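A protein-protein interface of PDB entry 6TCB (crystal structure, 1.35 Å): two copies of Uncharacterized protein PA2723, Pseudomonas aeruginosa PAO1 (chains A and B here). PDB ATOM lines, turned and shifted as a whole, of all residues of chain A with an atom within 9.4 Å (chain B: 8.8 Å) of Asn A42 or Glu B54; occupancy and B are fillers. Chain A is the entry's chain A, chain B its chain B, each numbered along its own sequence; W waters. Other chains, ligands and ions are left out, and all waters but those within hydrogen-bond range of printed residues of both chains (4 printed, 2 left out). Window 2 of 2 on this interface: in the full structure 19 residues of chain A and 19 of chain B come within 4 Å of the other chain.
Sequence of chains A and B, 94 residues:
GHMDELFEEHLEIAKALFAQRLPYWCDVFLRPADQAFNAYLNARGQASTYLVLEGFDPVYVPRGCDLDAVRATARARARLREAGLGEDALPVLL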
ATOM      1  N   PHE A   7     -13.664   2.535  -2.515  1.00  0.00           N
ATOM      2  CA  PHE A   7     -13.650   1.090  -2.705  1.00  0.00           C
ATOM      3  C   PHE A   7     -14.260   0.365  -1.510  1.00  0.00           C
ATOM      4  O   PHE A   7     -15.008  -0.603  -1.685  1.00  0.00           O
ATOM      5  CB  PHE A   7     -12.222   0.611  -2.960  1.00  0.00           C
ATOM      6  CG  PHE A   7     -11.808   0.636  -4.414  1.00  0.00           C
ATOM      7  CD1 PHE A   7     -12.370   1.516  -5.321  1.00  0.00           C
ATOM      8  CD2 PHE A   7     -10.865  -0.256  -4.871  1.00  0.00           C
ATOM      9  CE1 PHE A   7     -11.973   1.498  -6.651  1.00  0.00           C
ATOM     10  CE2 PHE A   7     -10.481  -0.287  -6.194  1.00  0.00           C
ATOM     11  CZ  PHE A   7     -11.020   0.597  -7.081  1.00  0.00           C
ATOM     12  N   LEU A  11     -17.533  -1.881  -1.775  1.00  0.00           N
ATOM     13  CA  LEU A  11     -17.439  -3.278  -1.361  1.00  0.00           C
ATOM     14  C   LEU A  11     -18.633  -3.659  -0.496  1.00  0.00           C
ATOM     15  O   LEU A  11     -19.168  -4.765  -0.615  1.00  0.00           O
ATOM     16  CB  LEU A  11     -16.136  -3.519  -0.599  1.00  0.00           C
ATOM     17  CG  LEU A  11     -16.007  -4.818   0.204  1.00  0.00           C
ATOM     18  CD1 LEU A  11     -15.971  -6.024  -0.693  1.00  0.00           C
ATOM     19  CD2 LEU A  11     -14.756  -4.771   1.110  1.00  0.00           C
ATOM     20  N   ALA A  14     -21.533  -4.174  -2.804  1.00  0.00           N
ATOM     21  CA  ALA A  14     -21.337  -5.450  -3.475  1.00  0.00           C
ATOM     22  C   ALA A  14     -21.654  -6.620  -2.555  1.00  0.00           C
ATOM     23  O   ALA A  14     -22.338  -7.563  -2.956  1.00  0.00           O
ATOM     24  CB  ALA A  14     -19.893  -5.565  -3.964  1.00  0.00           C
ATOM     25  N   PHE A  18     -24.004  -9.667  -3.302  1.00  0.00           N
ATOM     26  CA  PHE A  18     -23.363 -10.963  -3.446  1.00  0.00           C
ATOM     27  C   PHE A  18     -23.937 -11.966  -2.451  1.00  0.00           C
ATOM     28  O   PHE A  18     -23.918 -13.172  -2.708  1.00  0.00           O
ATOM     29  CB  PHE A  18     -21.855 -10.850  -3.248  1.00  0.00           C
ATOM     30  CG  PHE A  18     -21.096 -10.200  -4.388  1.00  0.00           C
ATOM     31  CD1 PHE A  18     -21.727  -9.615  -5.485  1.00  0.00           C
ATOM     32  CD2 PHE A  18     -19.721 -10.180  -4.332  1.00  0.00           C
ATOM     33  CE1 PHE A  18     -20.988  -9.031  -6.489  1.00  0.00           C
ATOM     34  CE2 PHE A  18     -18.978  -9.611  -5.333  1.00  0.00           C
ATOM     35  CZ  PHE A  18     -19.615  -9.033  -6.414  1.00  0.00           C
ATOM     36  N   GLN A  35     -11.666  -1.679 -13.481  1.00  0.00           N
ATOM     37  CA  GLN A  35     -11.139  -3.040 -13.484  1.00  0.00           C
ATOM     38  C   GLN A  35     -10.496  -3.380 -12.149  1.00  0.00           C
ATOM     39  O   GLN A  35     -10.614  -4.514 -11.660  1.00  0.00           O
ATOM     40  CB  GLN A  35     -10.111  -3.184 -14.605  1.00  0.00           C
ATOM     41  CG  GLN A  35     -10.684  -2.937 -15.987  1.00  0.00           C
ATOM     42  CD  GLN A  35      -9.764  -3.409 -17.093  1.00  0.00           C
ATOM     43  OE1 GLN A  35      -9.545  -4.612 -17.253  1.00  0.00           O
ATOM     44  NE2 GLN A  35      -9.222  -2.470 -17.863  1.00  0.00           N
ATOM     45  N   ALA A  36      -9.824  -2.406 -11.539  1.00  0.00           N
ATOM     46  CA  ALA A  36      -9.135  -2.646 -10.281  1.00  0.00           C
ATOM     47  C   ALA A  36     -10.111  -2.981  -9.170  1.00  0.00           C
ATOM     48  O   ALA A  36      -9.761  -3.725  -8.249  1.00  0.00           O
ATOM     49  CB  ALA A  36      -8.307  -1.421  -9.905  1.00  0.00           C
ATOM     50  N   PHE A  37     -11.337  -2.453  -9.233  1.00  0.00           N
ATOM     51  CA  PHE A  37     -12.310  -2.812  -8.208  1.00  0.00           C
ATOM     52  C   PHE A  37     -12.529  -4.320  -8.159  1.00  0.00           C
ATOM     53  O   PHE A  37     -12.792  -4.869  -7.086  1.00  0.00           O
ATOM     54  CB  PHE A  37     -13.632  -2.056  -8.402  1.00  0.00           C
ATOM     55  CG  PHE A  37     -14.618  -2.261  -7.277  1.00  0.00           C
ATOM     56  CD1 PHE A  37     -14.326  -1.803  -6.006  1.00  0.00           C
ATOM     57  CD2 PHE A  37     -15.834  -2.895  -7.503  1.00  0.00           C
ATOM     58  CE1 PHE A  37     -15.216  -1.986  -4.967  1.00  0.00           C
ATOM     59  CE2 PHE A  37     -16.735  -3.083  -6.468  1.00  0.00           C
ATOM     60  CZ  PHE A  37     -16.425  -2.631  -5.207  1.00  0.00           C
ATOM     61  N   ASN A  38     -12.424  -5.014  -9.299  1.00  0.00           N
ATOM     62  CA  ASN A  38     -12.574  -6.463  -9.246  1.00  0.00           C
ATOM     63  C   ASN A  38     -11.436  -7.113  -8.467  1.00  0.00           C
ATOM     64  O   ASN A  38     -11.654  -8.083  -7.729  1.00  0.00           O
ATOM     65  CB  ASN A  38     -12.699  -7.064 -10.639  1.00  0.00           C
ATOM     66  CG  ASN A  38     -13.394  -8.392 -10.605  1.00  0.00           C
ATOM     67  OD1 ASN A  38     -14.558  -8.476 -10.221  1.00  0.00           O
ATOM     68  ND2 ASN A  38     -12.688  -9.444 -10.988  1.00  0.00           N
ATOM     69  N   ALA A  39     -10.222  -6.576  -8.597  1.00  0.00           N
ATOM     70  CA  ALA A  39      -9.108  -7.086  -7.801  1.00  0.00           C
ATOM     71  C   ALA A  39      -9.338  -6.829  -6.318  1.00  0.00           C
ATOM     72  O   ALA A  39      -8.975  -7.656  -5.473  1.00  0.00           O
ATOM     73  CB  ALA A  39      -7.796  -6.451  -8.266  1.00  0.00           C
ATOM     74  N   TYR A  40      -9.934  -5.679  -5.987  1.00  0.00           N
ATOM     75  CA  TYR A  40     -10.246  -5.339  -4.607  1.00  0.00           C
ATOM     76  C   TYR A  40     -11.256  -6.316  -4.028  1.00  0.00           C
ATOM     77  O   TYR A  40     -11.069  -6.846  -2.928  1.00  0.00           O
ATOM     78  CB  TYR A  40     -10.802  -3.909  -4.549  1.00  0.00           C
ATOM     79  CG  TYR A  40     -10.948  -3.362  -3.147  1.00  0.00           C
ATOM     80  CD1 TYR A  40      -9.839  -2.952  -2.429  1.00  0.00           C
ATOM     81  CD2 TYR A  40     -12.195  -3.252  -2.541  1.00  0.00           C
ATOM     82  CE1 TYR A  40      -9.956  -2.454  -1.128  1.00  0.00           C
ATOM     83  CE2 TYR A  40     -12.317  -2.767  -1.259  1.00  0.00           C
ATOM     84  CZ  TYR A  40     -11.202  -2.362  -0.562  1.00  0.00           C
ATOM     85  OH  TYR A  40     -11.339  -1.869   0.715  1.00  0.00           O
ATOM     86  N   LEU A  41     -12.348  -6.559  -4.758  1.00  0.00           N
ATOM     87  CA  LEU A  41     -13.341  -7.527  -4.302  1.00  0.00           C
ATOM     88  C   LEU A  41     -12.697  -8.879  -4.016  1.00  0.00           C
ATOM     89  O   LEU A  41     -12.892  -9.464  -2.947  1.00  0.00           O
ATOM     90  CB  LEU A  41     -14.435  -7.677  -5.358  1.00  0.00           C
ATOM     91  CG  LEU A  41     -15.390  -6.493  -5.507  1.00  0.00           C
ATOM     92  CD1 LEU A  41     -16.241  -6.697  -6.737  1.00  0.00           C
ATOM     93  CD2 LEU A  41     -16.254  -6.273  -4.266  1.00  0.00           C
ATOM     94  N   ASN A  42     -11.894  -9.379  -4.956  1.00  0.00           N
ATOM     95  CA  ASN A  42     -11.284 -10.695  -4.777  1.00  0.00           C
ATOM     96  C   ASN A  42     -10.301 -10.700  -3.615  1.00  0.00           C
ATOM     97  O   ASN A  42     -10.266 -11.656  -2.835  1.00  0.00           O
ATOM     98  CB  ASN A  42     -10.634 -11.158  -6.085  1.00  0.00           C
ATOM     99  CG  ASN A  42     -11.655 -11.678  -7.085  1.00  0.00           C
ATOM    100  OD1 ASN A  42     -12.256 -12.734  -6.883  1.00  0.00           O
ATOM    101  ND2 ASN A  42     -11.869 -10.941  -8.154  1.00  0.00           N
ATOM    102  N   ALA A  43      -9.517  -9.636  -3.462  1.00  0.00           N
ATOM    103  CA  ALA A  43      -8.572  -9.590  -2.352  1.00  0.00           C
ATOM    104  C   ALA A  43      -9.278  -9.576  -1.006  1.00  0.00           C
ATOM    105  O   ALA A  43      -8.756 -10.130  -0.028  1.00  0.00           O
ATOM    106  CB  ALA A  43      -7.687  -8.351  -2.483  1.00  0.00           C
ATOM    107  N   ARG A  44     -10.456  -8.942  -0.927  1.00  0.00           N
ATOM    108  CA  ARG A  44     -11.203  -8.813   0.311  1.00  0.00           C
ATOM    109  C   ARG A  44     -12.153  -9.985   0.549  1.00  0.00           C
ATOM    110  O   ARG A  44     -13.014  -9.901   1.433  1.00  0.00           O
ATOM    111  CB  ARG A  44     -12.007  -7.507   0.335  1.00  0.00           C
ATOM    112  CG  ARG A  44     -11.248  -6.222   0.051  1.00  0.00           C
ATOM    113  CD  ARG A  44     -10.192  -5.894   1.088  1.00  0.00           C
ATOM    114  NE  ARG A  44     -10.514  -6.350   2.435  1.00  0.00           N
ATOM    115  CZ  ARG A  44     -11.268  -5.682   3.303  1.00  0.00           C
ATOM    116  NH1 ARG A  44     -11.481  -6.188   4.510  1.00  0.00           N
ATOM    117  NH2 ARG A  44     -11.818  -4.522   2.968  1.00  0.00           N
ATOM    118  N   GLY A  45     -12.037 -11.059  -0.232  1.00  0.00           N
ATOM    119  CA  GLY A  45     -12.756 -12.286   0.041  1.00  0.00           C
ATOM    120  C   GLY A  45     -14.092 -12.431  -0.648  1.00  0.00           C
ATOM    121  O   GLY A  45     -14.870 -13.320  -0.278  1.00  0.00           O
ATOM    122  N   GLN A  46     -14.373 -11.605  -1.641  1.00  0.00           N
ATOM    123  CA  GLN A  46     -15.629 -11.617  -2.379  1.00  0.00           C
ATOM    124  C   GLN A  46     -15.303 -12.038  -3.803  1.00  0.00           C
ATOM    125  O   GLN A  46     -15.010 -11.198  -4.654  1.00  0.00           O
ATOM    126  CB  GLN A  46     -16.262 -10.230  -2.360  1.00  0.00           C
ATOM    127  CG  GLN A  46     -16.710  -9.774  -0.990  1.00  0.00           C
ATOM    128  CD  GLN A  46     -17.749 -10.696  -0.392  1.00  0.00           C
ATOM    129  OE1 GLN A  46     -18.770 -10.988  -1.013  1.00  0.00           O
ATOM    130  NE2 GLN A  46     -17.502 -11.149   0.824  1.00  0.00           N
ATOM    131  N   ALA A  47     -15.352 -13.349  -4.054  1.00  0.00           N
ATOM    132  CA  ALA A  47     -14.988 -13.887  -5.357  1.00  0.00           C
ATOM    133  C   ALA A  47     -15.866 -13.277  -6.436  1.00  0.00           C
ATOM    134  O   ALA A  47     -17.096 -13.316  -6.347  1.00  0.00           O
ATOM    135  CB  ALA A  47     -15.158 -15.407  -5.346  1.00  0.00           C
ATOM    136  N   SER A  48     -15.230 -12.708  -7.455  1.00  0.00           N
ATOM    137  CA  SER A  48     -15.944 -11.906  -8.434  1.00  0.00           C
ATOM    138  C   SER A  48     -15.293 -11.975  -9.802  1.00  0.00           C
ATOM    139  O   SER A  48     -14.065 -11.964  -9.924  1.00  0.00           O
ATOM    140  CB  SER A  48     -15.972 -10.431  -7.981  1.00  0.00           C
ATOM    141  OG  SER A  48     -16.660  -9.612  -8.911  1.00  0.00           O
ATOM    142  N   THR A  49     -16.148 -12.010 -10.821  1.00  0.00           N
ATOM    143  CA  THR A  49     -15.761 -11.866 -12.219  1.00  0.00           C
ATOM    144  C   THR A  49     -16.250 -10.518 -12.732  1.00  0.00           C
ATOM    145  O   THR A  49     -17.421 -10.165 -12.558  1.00  0.00           O
ATOM    146  CB  THR A  49     -16.401 -12.981 -13.051  1.00  0.00           C
ATOM    147  OG1 THR A  49     -16.001 -14.248 -12.522  1.00  0.00           O
ATOM    148  CG2 THR A  49     -15.977 -12.891 -14.510  1.00  0.00           C
ATOM    149  N   TYR A  50     -15.374  -9.779 -13.391  1.00  0.00           N
ATOM    150  CA  TYR A  50     -15.732  -8.500 -13.981  1.00  0.00           C
ATOM    151  C   TYR A  50     -16.116  -8.708 -15.431  1.00  0.00           C
ATOM    152  O   TYR A  50     -15.393  -9.383 -16.176  1.00  0.00           O
ATOM    153  CB  TYR A  50     -14.544  -7.559 -13.904  1.00  0.00           C
ATOM    154  CG  TYR A  50     -14.687  -6.205 -14.548  1.00  0.00           C
ATOM    155  CD1 TYR A  50     -15.578  -5.261 -14.059  1.00  0.00           C
ATOM    156  CD2 TYR A  50     -13.863  -5.849 -15.599  1.00  0.00           C
ATOM    157  CE1 TYR A  50     -15.660  -4.005 -14.629  1.00  0.00           C
ATOM    158  CE2 TYR A  50     -13.938  -4.595 -16.174  1.00  0.00           C
ATOM    159  CZ  TYR A  50     -14.831  -3.672 -15.660  1.00  0.00           C
ATOM    160  OH  TYR A  50     -14.903  -2.411 -16.218  1.00  0.00           O
ATOM    161  N   TYR A  60     -19.911  -6.606 -11.693  1.00  0.00           N
ATOM    162  CA  TYR A  60     -19.087  -7.469 -10.857  1.00  0.00           C
ATOM    163  C   TYR A  60     -19.984  -8.621 -10.428  1.00  0.00           C
ATOM    164  O   TYR A  60     -21.016  -8.393  -9.791  1.00  0.00           O
ATOM    165  CB  TYR A  60     -18.539  -6.675  -9.660  1.00  0.00           C
ATOM    166  CG  TYR A  60     -17.816  -5.429 -10.120  1.00  0.00           C
ATOM    167  CD1 TYR A  60     -16.473  -5.464 -10.443  1.00  0.00           C
ATOM    168  CD2 TYR A  60     -18.488  -4.221 -10.294  1.00  0.00           C
ATOM    169  CE1 TYR A  60     -15.818  -4.338 -10.910  1.00  0.00           C
ATOM    170  CE2 TYR A  60     -17.832  -3.084 -10.762  1.00  0.00           C
ATOM    171  CZ  TYR A  60     -16.501  -3.160 -11.080  1.00  0.00           C
ATOM    172  OH  TYR A  60     -15.903  -2.006 -11.538  1.00  0.00           O
ATOM    173  N   VAL A  61     -19.641  -9.829 -10.843  1.00  0.00           N
ATOM    174  CA  VAL A  61     -20.533 -10.983 -10.752  1.00  0.00           C
ATOM    175  C   VAL A  61     -19.963 -11.966  -9.738  1.00  0.00           C
ATOM    176  O   VAL A  61     -18.843 -12.463  -9.933  1.00  0.00           O
ATOM    177  CB  VAL A  61     -20.714 -11.674 -12.112  1.00  0.00           C
ATOM    178  CG1 VAL A  61     -21.738 -12.792 -11.975  1.00  0.00           C
ATOM    179  CG2 VAL A  61     -21.123 -10.679 -13.153  1.00  0.00           C
ATOM    180  N   PRO A  62     -20.700 -12.305  -8.683  1.00  0.00           N
ATOM    181  CA  PRO A  62     -20.185 -13.259  -7.700  1.00  0.00           C
ATOM    182  C   PRO A  62     -20.171 -14.680  -8.251  1.00  0.00           C
ATOM    183  O   PRO A  62     -20.968 -15.052  -9.113  1.00  0.00           O
ATOM    184  CB  PRO A  62     -21.183 -13.132  -6.542  1.00  0.00           C
ATOM    185  CG  PRO A  62     -22.483 -12.744  -7.232  1.00  0.00           C
ATOM    186  CD  PRO A  62     -22.093 -11.884  -8.405  1.00  0.00           C
ATOM    187  N   ARG A  63     -19.250 -15.489  -7.734  1.00  0.00           N
ATOM    188  CA  ARG A  63     -19.324 -16.929  -7.967  1.00  0.00           C
ATOM    189  C   ARG A  63     -20.689 -17.446  -7.519  1.00  0.00           C
ATOM    190  O   ARG A  63     -21.233 -17.014  -6.503  1.00  0.00           O
ATOM    191  CB  ARG A  63     -18.198 -17.619  -7.196  1.00  0.00           C
ATOM    192  CG  ARG A  63     -17.772 -18.963  -7.770  1.00  0.00           C
ATOM    193  CD  ARG A  63     -16.653 -19.601  -6.942  1.00  0.00           C
ATOM    194  N   ARG B  31      -3.223  -2.302 -20.098  1.00  0.00           N
ATOM    195  CA  ARG B  31      -4.367  -1.762 -19.381  1.00  0.00           C
ATOM    196  C   ARG B  31      -4.214  -0.245 -19.268  1.00  0.00           C
ATOM    197  O   ARG B  31      -3.119   0.240 -18.951  1.00  0.00           O
ATOM    198  CB  ARG B  31      -4.462  -2.383 -17.978  1.00  0.00           C
ATOM    199  CG  ARG B  31      -5.866  -2.294 -17.335  1.00  0.00           C
ATOM    200  CD  ARG B  31      -5.843  -2.086 -15.810  1.00  0.00           C
ATOM    201  NE  ARG B  31      -6.239  -3.244 -15.000  1.00  0.00           N
ATOM    202  CZ  ARG B  31      -6.680  -3.156 -13.743  1.00  0.00           C
ATOM    203  NH1 ARG B  31      -7.010  -4.243 -13.056  1.00  0.00           N
ATOM    204  NH2 ARG B  31      -6.804  -1.967 -13.174  1.00  0.00           N
ATOM    205  N   LEU B  51     -14.218  -9.875 -20.340  1.00  0.00           N
ATOM    206  CA  LEU B  51     -14.236 -10.623 -19.086  1.00  0.00           C
ATOM    207  C   LEU B  51     -12.861 -10.600 -18.435  1.00  0.00           C
ATOM    208  O   LEU B  51     -11.843 -10.792 -19.114  1.00  0.00           O
ATOM    209  CB  LEU B  51     -14.682 -12.076 -19.320  1.00  0.00           C
ATOM    210  CG  LEU B  51     -14.705 -13.024 -18.118  1.00  0.00           C
ATOM    211  CD1 LEU B  51     -15.711 -14.137 -18.428  1.00  0.00           C
ATOM    212  CD2 LEU B  51     -13.368 -13.653 -17.751  1.00  0.00           C
ATOM    213  N   VAL B  52     -12.839 -10.345 -17.128  1.00  0.00           N
ATOM    214  CA  VAL B  52     -11.618 -10.339 -16.332  1.00  0.00           C
ATOM    215  C   VAL B  52     -11.865 -11.111 -15.045  1.00  0.00           C
ATOM    216  O   VAL B  52     -12.814 -10.817 -14.309  1.00  0.00           O
ATOM    217  CB  VAL B  52     -11.169  -8.909 -15.989  1.00  0.00           C
ATOM    218  CG1 VAL B  52      -9.899  -8.962 -15.169  1.00  0.00           C
ATOM    219  CG2 VAL B  52     -10.950  -8.102 -17.245  1.00  0.00           C
ATOM    220  N   LEU B  53     -10.966 -12.041 -14.723  1.00  0.00           N
ATOM    221  CA  LEU B  53     -11.086 -12.847 -13.506  1.00  0.00           C
ATOM    222  C   LEU B  53     -10.097 -12.341 -12.456  1.00  0.00           C
ATOM    223  O   LEU B  53     -10.415 -11.390 -11.736  1.00  0.00           O
ATOM    224  CB  LEU B  53     -10.965 -14.337 -13.837  1.00  0.00           C
ATOM    225  CG  LEU B  53     -11.197 -15.400 -12.756  1.00  0.00           C
ATOM    226  CD1 LEU B  53     -12.585 -15.334 -12.129  1.00  0.00           C
ATOM    227  CD2 LEU B  53     -10.957 -16.806 -13.325  1.00  0.00           C
ATOM    228  N   GLU B  54      -8.905 -12.930 -12.346  1.00  0.00           N
ATOM    229  CA  GLU B  54      -7.988 -12.513 -11.289  1.00  0.00           C
ATOM    230  C   GLU B  54      -6.552 -12.246 -11.726  1.00  0.00           C
ATOM    231  O   GLU B  54      -5.715 -11.939 -10.870  1.00  0.00           O
ATOM    232  CB  GLU B  54      -7.987 -13.527 -10.131  1.00  0.00           C
ATOM    233  CG  GLU B  54      -9.095 -13.318  -9.110  1.00  0.00           C
ATOM    234  CD  GLU B  54      -9.089 -14.378  -8.025  1.00  0.00           C
ATOM    235  OE1 GLU B  54      -9.040 -15.577  -8.368  1.00  0.00           O
ATOM    236  OE2 GLU B  54      -9.121 -14.012  -6.830  1.00  0.00           O
ATOM    237  N   GLY B  55      -6.241 -12.341 -13.020  1.00  0.00           N
ATOM    238  CA  GLY B  55      -4.919 -12.015 -13.514  1.00  0.00           C
ATOM    239  C   GLY B  55      -5.019 -11.207 -14.792  1.00  0.00           C
ATOM    240  O   GLY B  55      -6.118 -10.933 -15.281  1.00  0.00           O
ATOM    241  N   PHE B  56      -3.857 -10.820 -15.324  1.00  0.00           N
ATOM    242  CA  PHE B  56      -3.837 -10.158 -16.627  1.00  0.00           C
ATOM    243  C   PHE B  56      -3.968 -11.233 -17.697  1.00  0.00           C
ATOM    244  O   PHE B  56      -3.005 -11.934 -18.029  1.00  0.00           O
ATOM    245  CB  PHE B  56      -2.598  -9.316 -16.888  1.00  0.00           C
ATOM    246  CG  PHE B  56      -2.631  -8.616 -18.235  1.00  0.00           C
ATOM    247  CD1 PHE B  56      -3.524  -7.578 -18.473  1.00  0.00           C
ATOM    248  CD2 PHE B  56      -1.790  -9.010 -19.264  1.00  0.00           C
ATOM    249  CE1 PHE B  56      -3.564  -6.931 -19.704  1.00  0.00           C
ATOM    250  CE2 PHE B  56      -1.822  -8.365 -20.498  1.00  0.00           C
ATOM    251  CZ  PHE B  56      -2.715  -7.327 -20.719  1.00  0.00           C
ATOM    252  N   ASP B  57      -5.135 -11.307 -18.331  1.00  0.00           N
ATOM    253  CA  ASP B  57      -5.365 -12.268 -19.408  1.00  0.00           C
ATOM    254  C   ASP B  57      -6.561 -11.811 -20.233  1.00  0.00           C
ATOM    255  O   ASP B  57      -7.590 -12.499 -20.285  1.00  0.00           O
ATOM    256  CB  ASP B  57      -5.613 -13.647 -18.805  1.00  0.00           C
ATOM    257  CG  ASP B  57      -5.425 -14.761 -19.800  1.00  0.00           C
ATOM    258  OD1 ASP B  57      -5.046 -14.475 -20.955  1.00  0.00           O
ATOM    259  OD2 ASP B  57      -5.630 -15.937 -19.415  1.00  0.00           O
ATOM    260  N   ARG B  71     -15.053 -18.356 -18.270  1.00  0.00           N
ATOM    261  CA  ARG B  71     -14.584 -18.161 -16.904  1.00  0.00           C
ATOM    262  C   ARG B  71     -13.796 -19.380 -16.418  1.00  0.00           C
ATOM    263  O   ARG B  71     -12.713 -19.235 -15.846  1.00  0.00           O
ATOM    264  CB  ARG B  71     -15.757 -17.870 -15.967  1.00  0.00           C
ATOM    265  CG  ARG B  71     -15.319 -17.647 -14.520  1.00  0.00           C
ATOM    266  CD  ARG B  71     -16.499 -17.574 -13.561  1.00  0.00           C
ATOM    267  NE  ARG B  71     -16.075 -17.313 -12.187  1.00  0.00           N
ATOM    268  CZ  ARG B  71     -15.805 -18.252 -11.284  1.00  0.00           C
ATOM    269  NH1 ARG B  71     -15.429 -17.902 -10.062  1.00  0.00           N
ATOM    270  NH2 ARG B  71     -15.912 -19.538 -11.595  1.00  0.00           N
ATOM    271  N   ALA B  74     -10.452 -19.368 -18.038  1.00  0.00           N
ATOM    272  CA  ALA B  74      -9.534 -18.396 -17.450  1.00  0.00           C
ATOM    273  C   ALA B  74      -8.867 -18.968 -16.208  1.00  0.00           C
ATOM    274  O   ALA B  74      -7.671 -18.754 -15.981  1.00  0.00           O
ATOM    275  CB  ALA B  74     -10.272 -17.106 -17.094  1.00  0.00           C
ATOM    276  N   ARG B  75      -9.623 -19.702 -15.393  1.00  0.00           N
ATOM    277  CA  ARG B  75      -9.054 -20.303 -14.193  1.00  0.00           C
ATOM    278  C   ARG B  75      -7.987 -21.325 -14.563  1.00  0.00           C
ATOM    279  O   ARG B  75      -6.905 -21.360 -13.967  1.00  0.00           O
ATOM    280  CB  ARG B  75     -10.164 -20.954 -13.366  1.00  0.00           C
ATOM    281  N   ALA B  78      -4.802 -19.623 -15.818  1.00  0.00           N
ATOM    282  CA  ALA B  78      -4.000 -19.047 -14.742  1.00  0.00           C
ATOM    283  C   ALA B  78      -3.183 -20.117 -14.023  1.00  0.00           C
ATOM    284  O   ALA B  78      -2.003 -19.905 -13.723  1.00  0.00           O
ATOM    285  CB  ALA B  78      -4.909 -18.309 -13.761  1.00  0.00           C
ATOM    286  N   ARG B  81      -0.326 -21.157 -16.390  1.00  0.00           N
ATOM    287  CA  ARG B  81       0.658 -20.080 -16.453  1.00  0.00           C
ATOM    288  C   ARG B  81       1.550 -20.081 -15.223  1.00  0.00           C
ATOM    289  O   ARG B  81       2.773 -19.943 -15.331  1.00  0.00           O
ATOM    290  CB  ARG B  81      -0.098 -18.753 -16.569  1.00  0.00           C
ATOM    291  CG  ARG B  81       0.746 -17.498 -16.702  1.00  0.00           C
ATOM    292  CD  ARG B  81      -0.142 -16.237 -16.864  1.00  0.00           C
ATOM    293  NE  ARG B  81      -1.000 -16.312 -18.045  1.00  0.00           N
ATOM    294  CZ  ARG B  81      -2.333 -16.397 -18.035  1.00  0.00           C
ATOM    295  NH1 ARG B  81      -3.022 -16.390 -16.899  1.00  0.00           N
ATOM    296  NH2 ARG B  81      -2.980 -16.484 -19.184  1.00  0.00           N
HETATM  297  O   HOH W   1      -8.505  -6.341 -11.960  1.00  0.00           O
HETATM  298  O   HOH W   2      -7.590  -5.805 -15.722  1.00  0.00           O
HETATM  299  O   HOH W   3     -18.387 -15.077 -11.210  1.00  0.00           O
HETATM  300  O   HOH W   4     -15.866 -15.564  -9.691  1.00  0.00           O
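O of Leu B53 sits at hydrogen-bond distance from ND2 of Asn A38 (3.1 Å).
The guanidinium group (NH2) of Arg B31 lies close to the backbone NH (N) of Ala A36 (3.5 Å).
The backbone carbonyl oxygen of Tyr A50 sits at hydrogen-bond distance from the backbone NH of Val B52 (2.9 Å).
OD1 of Asn A42 sits close to OE2 of Glu B54.
The side-chain hydroxyl (OG1) of Thr A49 lies within hydrogen-bond range of the guanidinium group (NE) of Arg B71 (3.1 Å).
The backbone NH of Arg A63 lies within hydrogen-bond range of the backbone carbonyl oxygen of Ala A47 (3.4 Å).
The backbone carbonyl oxygen (O) of Thr A49 sits at hydrogen-bond distance from the backbone NH (N) of Val A61.
ND2 of Asn A42 lies within hydrogen-bond range of O of Ser A48 (3.0 Å).
The backbone carbonyl oxygen (O) of Asn A38 sits at hydrogen-bond distance from the side-chain amide nitrogen (ND2) of Asn A42 (2.9 Å).
The side-chain amide oxygen (OD1) of Asn A38 is in hydrogen-bond range of the side-chain hydroxyl (OG) of Ser A48 (2.7 Å).
Gln A35 touches Arg B31 (NE2 to CG, 3.4 Å).
Gln A35 touches Val B52.
Asn A38 touches Val B52 (ND2 to O, 3.6 Å).
O of Leu B53 touches ND2 of Asn A42, at 3.9 Å.
Thr A49 touches Leu B51 (CG2 to CG, 3.8 Å).
Thr A49 touches Val B52 (CA to O, 3.8 Å).
CD1 of Leu B53 touches OG1 of Thr A49, at 3.6 Å.
Tyr A50 touches Leu B51.
Arg B71 touches Arg A63 (NH1 to CG, 3.4 Å).
Of the printed residues of chain B, Gln A35 touches Arg B31 and Val B52.
Phe A37 touches none of the printed residues of chain B.
Asn A42 touches just these residues of chain B: Leu B53 and Glu B54.
No residue of chain B comes within 4 Å of Ala A43.
Of the printed residues of chain B, Arg A63 touches Arg B71.
Printed residues of chain A within 4 Å of Arg B31: Gln A35 and Ala A36.
Of chain A, only Asn A38, Asn A42 and Thr A49 come within 4 Å of Leu B53.
Of the printed residues of chain A, Glu B54 touches Asn A42 (3.3 Å).
Phe B56 touches none of the printed residues of chain A.
The nearest residue of chain B that does not touch Asn A42 is Val B52 (6.2 Å).
The nearest residue of chain A that does not touch Glu B54 is Ser A48 (5.2 Å).
Of the 13 printed residues of chain B, 6 touch a printed residue of chain A.
Hydrophobic or aromatic side chains of chain B that line the printed part of chain A: Leu B51, Val B52 and Leu B53.
Among the printed residues, 14 pairs touch across the chains.
Among the printed residues, no Asp or Glu carboxylate lies within 4 Å of a Lys or Arg side-chain nitrogen of the other chain.
No position is printed for both chains.
Of the 14 pairs that touch across the chains among the printed residues, none has its exchanged pair printed and touching as well.
Water W4 bridges NH1 of Arg B71 (2.4 Å) and OG1 of Thr A49 (3.1 Å).
Water W2 bridges the side-chain amide oxygen (OE1) of Gln A35 (2.8 Å) and the guanidinium group (NE) of Arg B31 (3.0 Å).
Water W1 lies within hydrogen-bond range of the guanidinium group (NH1) of Arg B31 (2.8 Å) and the backbone carbonyl oxygen (O) of Gln A35 (2.8 Å).
Water W3 lies within hydrogen-bond range of the side-chain hydroxyl of Thr A49 (2.8 Å), the backbone carbonyl oxygen of Val A61 (2.9 Å), the backbone carbonyl oxygen of Pro A62 (3.3 Å) and the guanidinium group of Arg B71 (3.4 Å).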
